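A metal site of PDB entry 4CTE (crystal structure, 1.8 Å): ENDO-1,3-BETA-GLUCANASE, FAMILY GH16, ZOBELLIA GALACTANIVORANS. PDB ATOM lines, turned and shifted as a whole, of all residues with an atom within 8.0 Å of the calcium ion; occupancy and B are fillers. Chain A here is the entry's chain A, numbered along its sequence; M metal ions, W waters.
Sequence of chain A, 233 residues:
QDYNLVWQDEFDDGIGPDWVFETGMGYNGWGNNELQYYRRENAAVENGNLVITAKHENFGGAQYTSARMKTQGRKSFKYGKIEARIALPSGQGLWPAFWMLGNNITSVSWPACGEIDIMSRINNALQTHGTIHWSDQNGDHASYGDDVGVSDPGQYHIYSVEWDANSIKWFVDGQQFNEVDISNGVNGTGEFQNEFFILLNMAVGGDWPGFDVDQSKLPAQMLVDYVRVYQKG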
ATOM      1  N   ASP A   9     -12.056   8.084   8.130  1.00  0.00           N
ATOM      2  CA  ASP A   9     -11.120   9.114   8.428  1.00  0.00           C
ATOM      3  C   ASP A   9     -10.672   8.743   9.829  1.00  0.00           C
ATOM      4  O   ASP A   9     -11.422   8.837  10.790  1.00  0.00           O
ATOM      5  CB  ASP A   9     -11.682  10.551   8.316  1.00  0.00           C
ATOM      6  CG  ASP A   9     -10.572  11.614   8.375  1.00  0.00           C
ATOM      7  OD1 ASP A   9      -9.463  11.335   8.863  1.00  0.00           O
ATOM      8  OD2 ASP A   9     -10.787  12.762   7.922  1.00  0.00           O
ATOM      9  N   GLU A  10      -9.437   8.276   9.916  1.00  0.00           N
ATOM     10  CA  GLU A  10      -8.842   7.791  11.166  1.00  0.00           C
ATOM     11  C   GLU A  10      -8.131   8.905  11.893  1.00  0.00           C
ATOM     12  O   GLU A  10      -7.707   8.691  13.024  1.00  0.00           O
ATOM     13  CB  GLU A  10      -7.860   6.637  10.909  1.00  0.00           C
ATOM     14  CG  GLU A  10      -8.487   5.416  10.236  1.00  0.00           C
ATOM     15  CD  GLU A  10      -9.570   4.731  11.070  1.00  0.00           C
ATOM     16  OE1 GLU A  10      -9.380   4.574  12.279  1.00  0.00           O
ATOM     17  OE2 GLU A  10     -10.606   4.323  10.514  1.00  0.00           O
ATOM     18  N   PHE A  11      -7.983  10.086  11.236  1.00  0.00           N
ATOM     19  CA  PHE A  11      -7.272  11.248  11.819  1.00  0.00           C
ATOM     20  C   PHE A  11      -5.878  10.846  12.362  1.00  0.00           C
ATOM     21  O   PHE A  11      -5.527  11.198  13.489  1.00  0.00           O
ATOM     22  CB  PHE A  11      -8.119  11.956  12.912  1.00  0.00           C
ATOM     23  CG  PHE A  11      -9.492  12.346  12.446  1.00  0.00           C
ATOM     24  CD1 PHE A  11      -9.642  13.410  11.508  1.00  0.00           C
ATOM     25  CD2 PHE A  11     -10.626  11.672  12.901  1.00  0.00           C
ATOM     26  CE1 PHE A  11     -10.884  13.774  11.037  1.00  0.00           C
ATOM     27  CE2 PHE A  11     -11.908  12.056  12.430  1.00  0.00           C
ATOM     28  CZ  PHE A  11     -12.014  13.108  11.487  1.00  0.00           C
ATOM     29  N   ASP A  12      -5.130  10.055  11.565  1.00  0.00           N
ATOM     30  CA  ASP A  12      -3.808   9.589  11.975  1.00  0.00           C
ATOM     31  C   ASP A  12      -2.797  10.723  12.132  1.00  0.00           C
ATOM     32  O   ASP A  12      -2.186  10.790  13.182  1.00  0.00           O
ATOM     33  CB  ASP A  12      -3.208   8.544  11.012  1.00  0.00           C
ATOM     34  CG  ASP A  12      -3.988   7.249  10.950  1.00  0.00           C
ATOM     35  OD1 ASP A  12      -4.574   6.802  11.939  1.00  0.00           O
ATOM     36  OD2 ASP A  12      -3.958   6.623   9.869  1.00  0.00           O
ATOM     37  N   ASP A  13      -2.692  11.596  11.122  1.00  0.00           N
ATOM     38  CA  ASP A  13      -1.725  12.743  11.207  1.00  0.00           C
ATOM     39  C   ASP A  13      -2.291  14.116  10.932  1.00  0.00           C
ATOM     40  O   ASP A  13      -1.686  15.101  11.360  1.00  0.00           O
ATOM     41  CB  ASP A  13      -0.456  12.486  10.349  1.00  0.00           C
ATOM     42  CG  ASP A  13       0.699  11.988  11.186  1.00  0.00           C
ATOM     43  OD1 ASP A  13       0.512  11.891  12.416  1.00  0.00           O
ATOM     44  OD2 ASP A  13       1.788  11.715  10.632  1.00  0.00           O
ATOM     45  N   VAL A  45      -5.767  18.147  14.827  1.00  0.00           N
ATOM     46  CA  VAL A  45      -5.508  16.733  15.095  1.00  0.00           C
ATOM     47  C   VAL A  45      -4.419  16.608  16.170  1.00  0.00           C
ATOM     48  O   VAL A  45      -3.366  17.252  16.088  1.00  0.00           O
ATOM     49  CB  VAL A  45      -5.157  15.946  13.816  1.00  0.00           C
ATOM     50  CG1 VAL A  45      -4.703  14.504  14.120  1.00  0.00           C
ATOM     51  CG2 VAL A  45      -6.374  15.899  12.916  1.00  0.00           C
ATOM     52  N   GLU A  46      -4.696  15.777  17.162  1.00  0.00           N
ATOM     53  CA  GLU A  46      -3.741  15.486  18.218  1.00  0.00           C
ATOM     54  C   GLU A  46      -3.877  14.021  18.538  1.00  0.00           C
ATOM     55  O   GLU A  46      -5.004  13.500  18.659  1.00  0.00           O
ATOM     56  CB  GLU A  46      -3.999  16.281  19.498  1.00  0.00           C
ATOM     57  CG  GLU A  46      -3.945  17.815  19.407  1.00  0.00           C
ATOM     58  CD  GLU A  46      -4.334  18.478  20.723  1.00  0.00           C
ATOM     59  OE1 GLU A  46      -4.240  17.834  21.799  1.00  0.00           O
ATOM     60  OE2 GLU A  46      -4.734  19.660  20.668  1.00  0.00           O
ATOM     61  N   ASN A  47      -2.732  13.361  18.696  1.00  0.00           N
ATOM     62  CA  ASN A  47      -2.682  11.958  19.128  1.00  0.00           C
ATOM     63  C   ASN A  47      -3.659  11.055  18.398  1.00  0.00           C
ATOM     64  O   ASN A  47      -4.311  10.222  19.035  1.00  0.00           O
ATOM     65  CB  ASN A  47      -2.975  11.900  20.640  1.00  0.00           C
ATOM     66  CG  ASN A  47      -1.936  12.606  21.465  1.00  0.00           C
ATOM     67  OD1 ASN A  47      -0.743  12.306  21.383  1.00  0.00           O
ATOM     68  ND2 ASN A  47      -2.408  13.541  22.290  1.00  0.00           N
ATOM     69  N   GLY A  48      -3.816  11.265  17.096  1.00  0.00           N
ATOM     70  CA  GLY A  48      -4.701  10.423  16.290  1.00  0.00           C
ATOM     71  C   GLY A  48      -6.183  10.728  16.430  1.00  0.00           C
ATOM     72  O   GLY A  48      -7.015   9.878  16.028  1.00  0.00           O
ATOM     73  N   ASN A  49      -6.515  11.905  16.975  1.00  0.00           N
ATOM     74  CA  ASN A  49      -7.901  12.328  17.111  1.00  0.00           C
ATOM     75  C   ASN A  49      -8.153  13.657  16.456  1.00  0.00           C
ATOM     76  O   ASN A  49      -7.307  14.548  16.550  1.00  0.00           O
ATOM     77  CB  ASN A  49      -8.385  12.556  18.594  1.00  0.00           C
ATOM     78  CG  ASN A  49      -8.397  11.300  19.451  1.00  0.00           C
ATOM     79  OD1 ASN A  49      -9.441  10.719  19.679  1.00  0.00           O
ATOM     80  ND2 ASN A  49      -7.235  10.872  19.924  1.00  0.00           N
ATOM     81  N   LEU A  50      -9.320  13.810  15.826  1.00  0.00           N
ATOM     82  CA  LEU A  50      -9.817  15.119  15.541  1.00  0.00           C
ATOM     83  C   LEU A  50     -10.183  15.725  16.905  1.00  0.00           C
ATOM     84  O   LEU A  50     -10.847  15.045  17.772  1.00  0.00           O
ATOM     85  CB  LEU A  50     -11.076  15.065  14.701  1.00  0.00           C
ATOM     86  CG  LEU A  50     -11.833  16.388  14.487  1.00  0.00           C
ATOM     87  CD1 LEU A  50     -11.029  17.364  13.586  1.00  0.00           C
ATOM     88  CD2 LEU A  50     -13.214  16.046  13.925  1.00  0.00           C
ATOM     89  N   ARG A  85     -16.031   7.014  16.863  1.00  0.00           N
ATOM     90  CA  ARG A  85     -15.565   6.798  18.221  1.00  0.00           C
ATOM     91  C   ARG A  85     -15.255   8.168  18.818  1.00  0.00           C
ATOM     92  O   ARG A  85     -14.226   8.824  18.478  1.00  0.00           O
ATOM     93  CB  ARG A  85     -14.351   5.881  18.225  1.00  0.00           C
ATOM     94  CG  ARG A  85     -13.815   5.602  19.596  1.00  0.00           C
ATOM     95  CD  ARG A  85     -12.964   4.342  19.537  1.00  0.00           C
ATOM     96  NE  ARG A  85     -12.633   3.924  20.900  1.00  0.00           N
ATOM     97  CZ  ARG A  85     -11.497   4.195  21.531  1.00  0.00           C
ATOM     98  NH1 ARG A  85     -10.488   4.863  20.916  1.00  0.00           N
ATOM     99  NH2 ARG A  85     -11.348   3.753  22.784  1.00  0.00           N
ATOM    100  N   TYR A 156     -14.454   7.293  25.579  1.00  0.00           N
ATOM    101  CA  TYR A 156     -14.845   6.949  24.196  1.00  0.00           C
ATOM    102  C   TYR A 156     -16.045   6.010  24.148  1.00  0.00           C
ATOM    103  O   TYR A 156     -16.168   5.104  24.973  1.00  0.00           O
ATOM    104  CB  TYR A 156     -13.704   6.252  23.454  1.00  0.00           C
ATOM    105  CG  TYR A 156     -12.592   7.178  23.118  1.00  0.00           C
ATOM    106  CD1 TYR A 156     -12.727   8.112  22.047  1.00  0.00           C
ATOM    107  CD2 TYR A 156     -11.378   7.152  23.820  1.00  0.00           C
ATOM    108  CE1 TYR A 156     -11.680   8.984  21.699  1.00  0.00           C
ATOM    109  CE2 TYR A 156     -10.336   8.024  23.489  1.00  0.00           C
ATOM    110  CZ  TYR A 156     -10.493   8.932  22.442  1.00  0.00           C
ATOM    111  OH  TYR A 156      -9.483   9.810  22.096  1.00  0.00           O
ATOM    112  N   VAL A 224     -12.597  12.961  18.443  1.00  0.00           N
ATOM    113  CA  VAL A 224     -13.165  11.979  17.528  1.00  0.00           C
ATOM    114  C   VAL A 224     -11.978  11.148  17.087  1.00  0.00           C
ATOM    115  O   VAL A 224     -11.107  11.633  16.344  1.00  0.00           O
ATOM    116  CB  VAL A 224     -13.947  12.619  16.345  1.00  0.00           C
ATOM    117  CG1 VAL A 224     -14.593  11.553  15.462  1.00  0.00           C
ATOM    118  CG2 VAL A 224     -14.990  13.666  16.849  1.00  0.00           C
ATOM    119  N   ASP A 225     -11.936   9.905  17.546  1.00  0.00           N
ATOM    120  CA  ASP A 225     -10.861   8.975  17.128  1.00  0.00           C
ATOM    121  C   ASP A 225     -10.990   8.645  15.637  1.00  0.00           C
ATOM    122  O   ASP A 225      -9.970   8.547  14.907  1.00  0.00           O
ATOM    123  CB  ASP A 225     -10.892   7.738  18.021  1.00  0.00           C
ATOM    124  CG  ASP A 225      -9.717   6.802  17.787  1.00  0.00           C
ATOM    125  OD1 ASP A 225      -8.692   7.211  17.177  1.00  0.00           O
ATOM    126  OD2 ASP A 225      -9.831   5.660  18.250  1.00  0.00           O
ATOM    127  N   TYR A 226     -12.232   8.497  15.161  1.00  0.00           N
ATOM    128  CA  TYR A 226     -12.476   8.174  13.759  1.00  0.00           C
ATOM    129  C   TYR A 226     -13.936   8.294  13.384  1.00  0.00           C
ATOM    130  O   TYR A 226     -14.805   8.265  14.263  1.00  0.00           O
ATOM    131  CB  TYR A 226     -11.982   6.724  13.421  1.00  0.00           C
ATOM    132  CG  TYR A 226     -12.558   5.574  14.253  1.00  0.00           C
ATOM    133  CD1 TYR A 226     -13.909   5.166  14.090  1.00  0.00           C
ATOM    134  CD2 TYR A 226     -11.748   4.878  15.169  1.00  0.00           C
ATOM    135  CE1 TYR A 226     -14.457   4.120  14.846  1.00  0.00           C
ATOM    136  CE2 TYR A 226     -12.283   3.806  15.934  1.00  0.00           C
ATOM    137  CZ  TYR A 226     -13.626   3.436  15.755  1.00  0.00           C
ATOM    138  OH  TYR A 226     -14.155   2.420  16.474  1.00  0.00           O
ATOM    139  N   VAL A 227     -14.177   8.337  12.077  1.00  0.00           N
ATOM    140  CA  VAL A 227     -15.486   8.243  11.457  1.00  0.00           C
ATOM    141  C   VAL A 227     -15.243   7.125  10.419  1.00  0.00           C
ATOM    142  O   VAL A 227     -14.231   7.135   9.693  1.00  0.00           O
ATOM    143  CB  VAL A 227     -15.986   9.579  10.853  1.00  0.00           C
ATOM    144  CG1 VAL A 227     -17.358   9.433  10.245  1.00  0.00           C
ATOM    145  CG2 VAL A 227     -16.034  10.654  11.944  1.00  0.00           C
ATOM    146  N   ARG A 228     -16.139   6.156  10.425  1.00  0.00           N
ATOM    147  CA  ARG A 228     -16.085   5.014   9.491  1.00  0.00           C
ATOM    148  C   ARG A 228     -17.437   4.774   8.931  1.00  0.00           C
ATOM    149  O   ARG A 228     -18.456   4.958   9.637  1.00  0.00           O
ATOM    150  CB  ARG A 228     -15.603   3.760  10.192  1.00  0.00           C
ATOM    151  CG  ARG A 228     -14.152   3.829  10.576  1.00  0.00           C
ATOM    152  CD  ARG A 228     -13.789   2.604  11.375  1.00  0.00           C
ATOM    153  NE  ARG A 228     -12.420   2.746  11.856  1.00  0.00           N
ATOM    154  CZ  ARG A 228     -11.869   2.034  12.837  1.00  0.00           C
ATOM    155  NH1 ARG A 228     -12.552   1.084  13.466  1.00  0.00           N
ATOM    156  NH2 ARG A 228     -10.611   2.272  13.185  1.00  0.00           N
HETATM  157 CA    CA M   1      -7.749   7.886  15.165  1.00  0.00          CA
HETATM  158  O   HOH W   1      -5.795   6.825  16.381  1.00  0.00           O
HETATM  159  O   HOH W   2      -5.494   7.807  14.365  1.00  0.00           O
HETATM  160  O   HOH W   3      -8.260   5.736  14.377  1.00  0.00           O
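OD2 of Asp 225 is in salt-bridge range of NH1 of Arg 85 (2.9 Å). N of Asp 225 is in hydrogen-bond range of OD1 of Asn 49 (3.4 Å). The guanidinium group (NE) of Arg 228 is in salt-bridge range of the side-chain carboxylate (OE2) of Glu 10, at 2.8 Å.
Of the 18 residues printed, 3 come within 4 Å of the calcium ion. The nearest printed residue that does not touch the calcium ion is Phe 11 (4.3 Å).
The backbone carbonyl oxygen (O) of Glu 10 is bound to the calcium ion. O of Gly 48 binds the calcium ion (2.3 Å). The calcium ion is bound by the side-chain carboxylate (OD1) of Asp 225 (2.3 Å). O of Asp 225 binds the calcium ion. The calcium ion is bound by water W3 (2.3 Å). Water W2 binds the calcium ion. Water W1 is bound to the calcium ion, at 2.5 Å. The calcium ion has seven donor atoms within binding distance.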
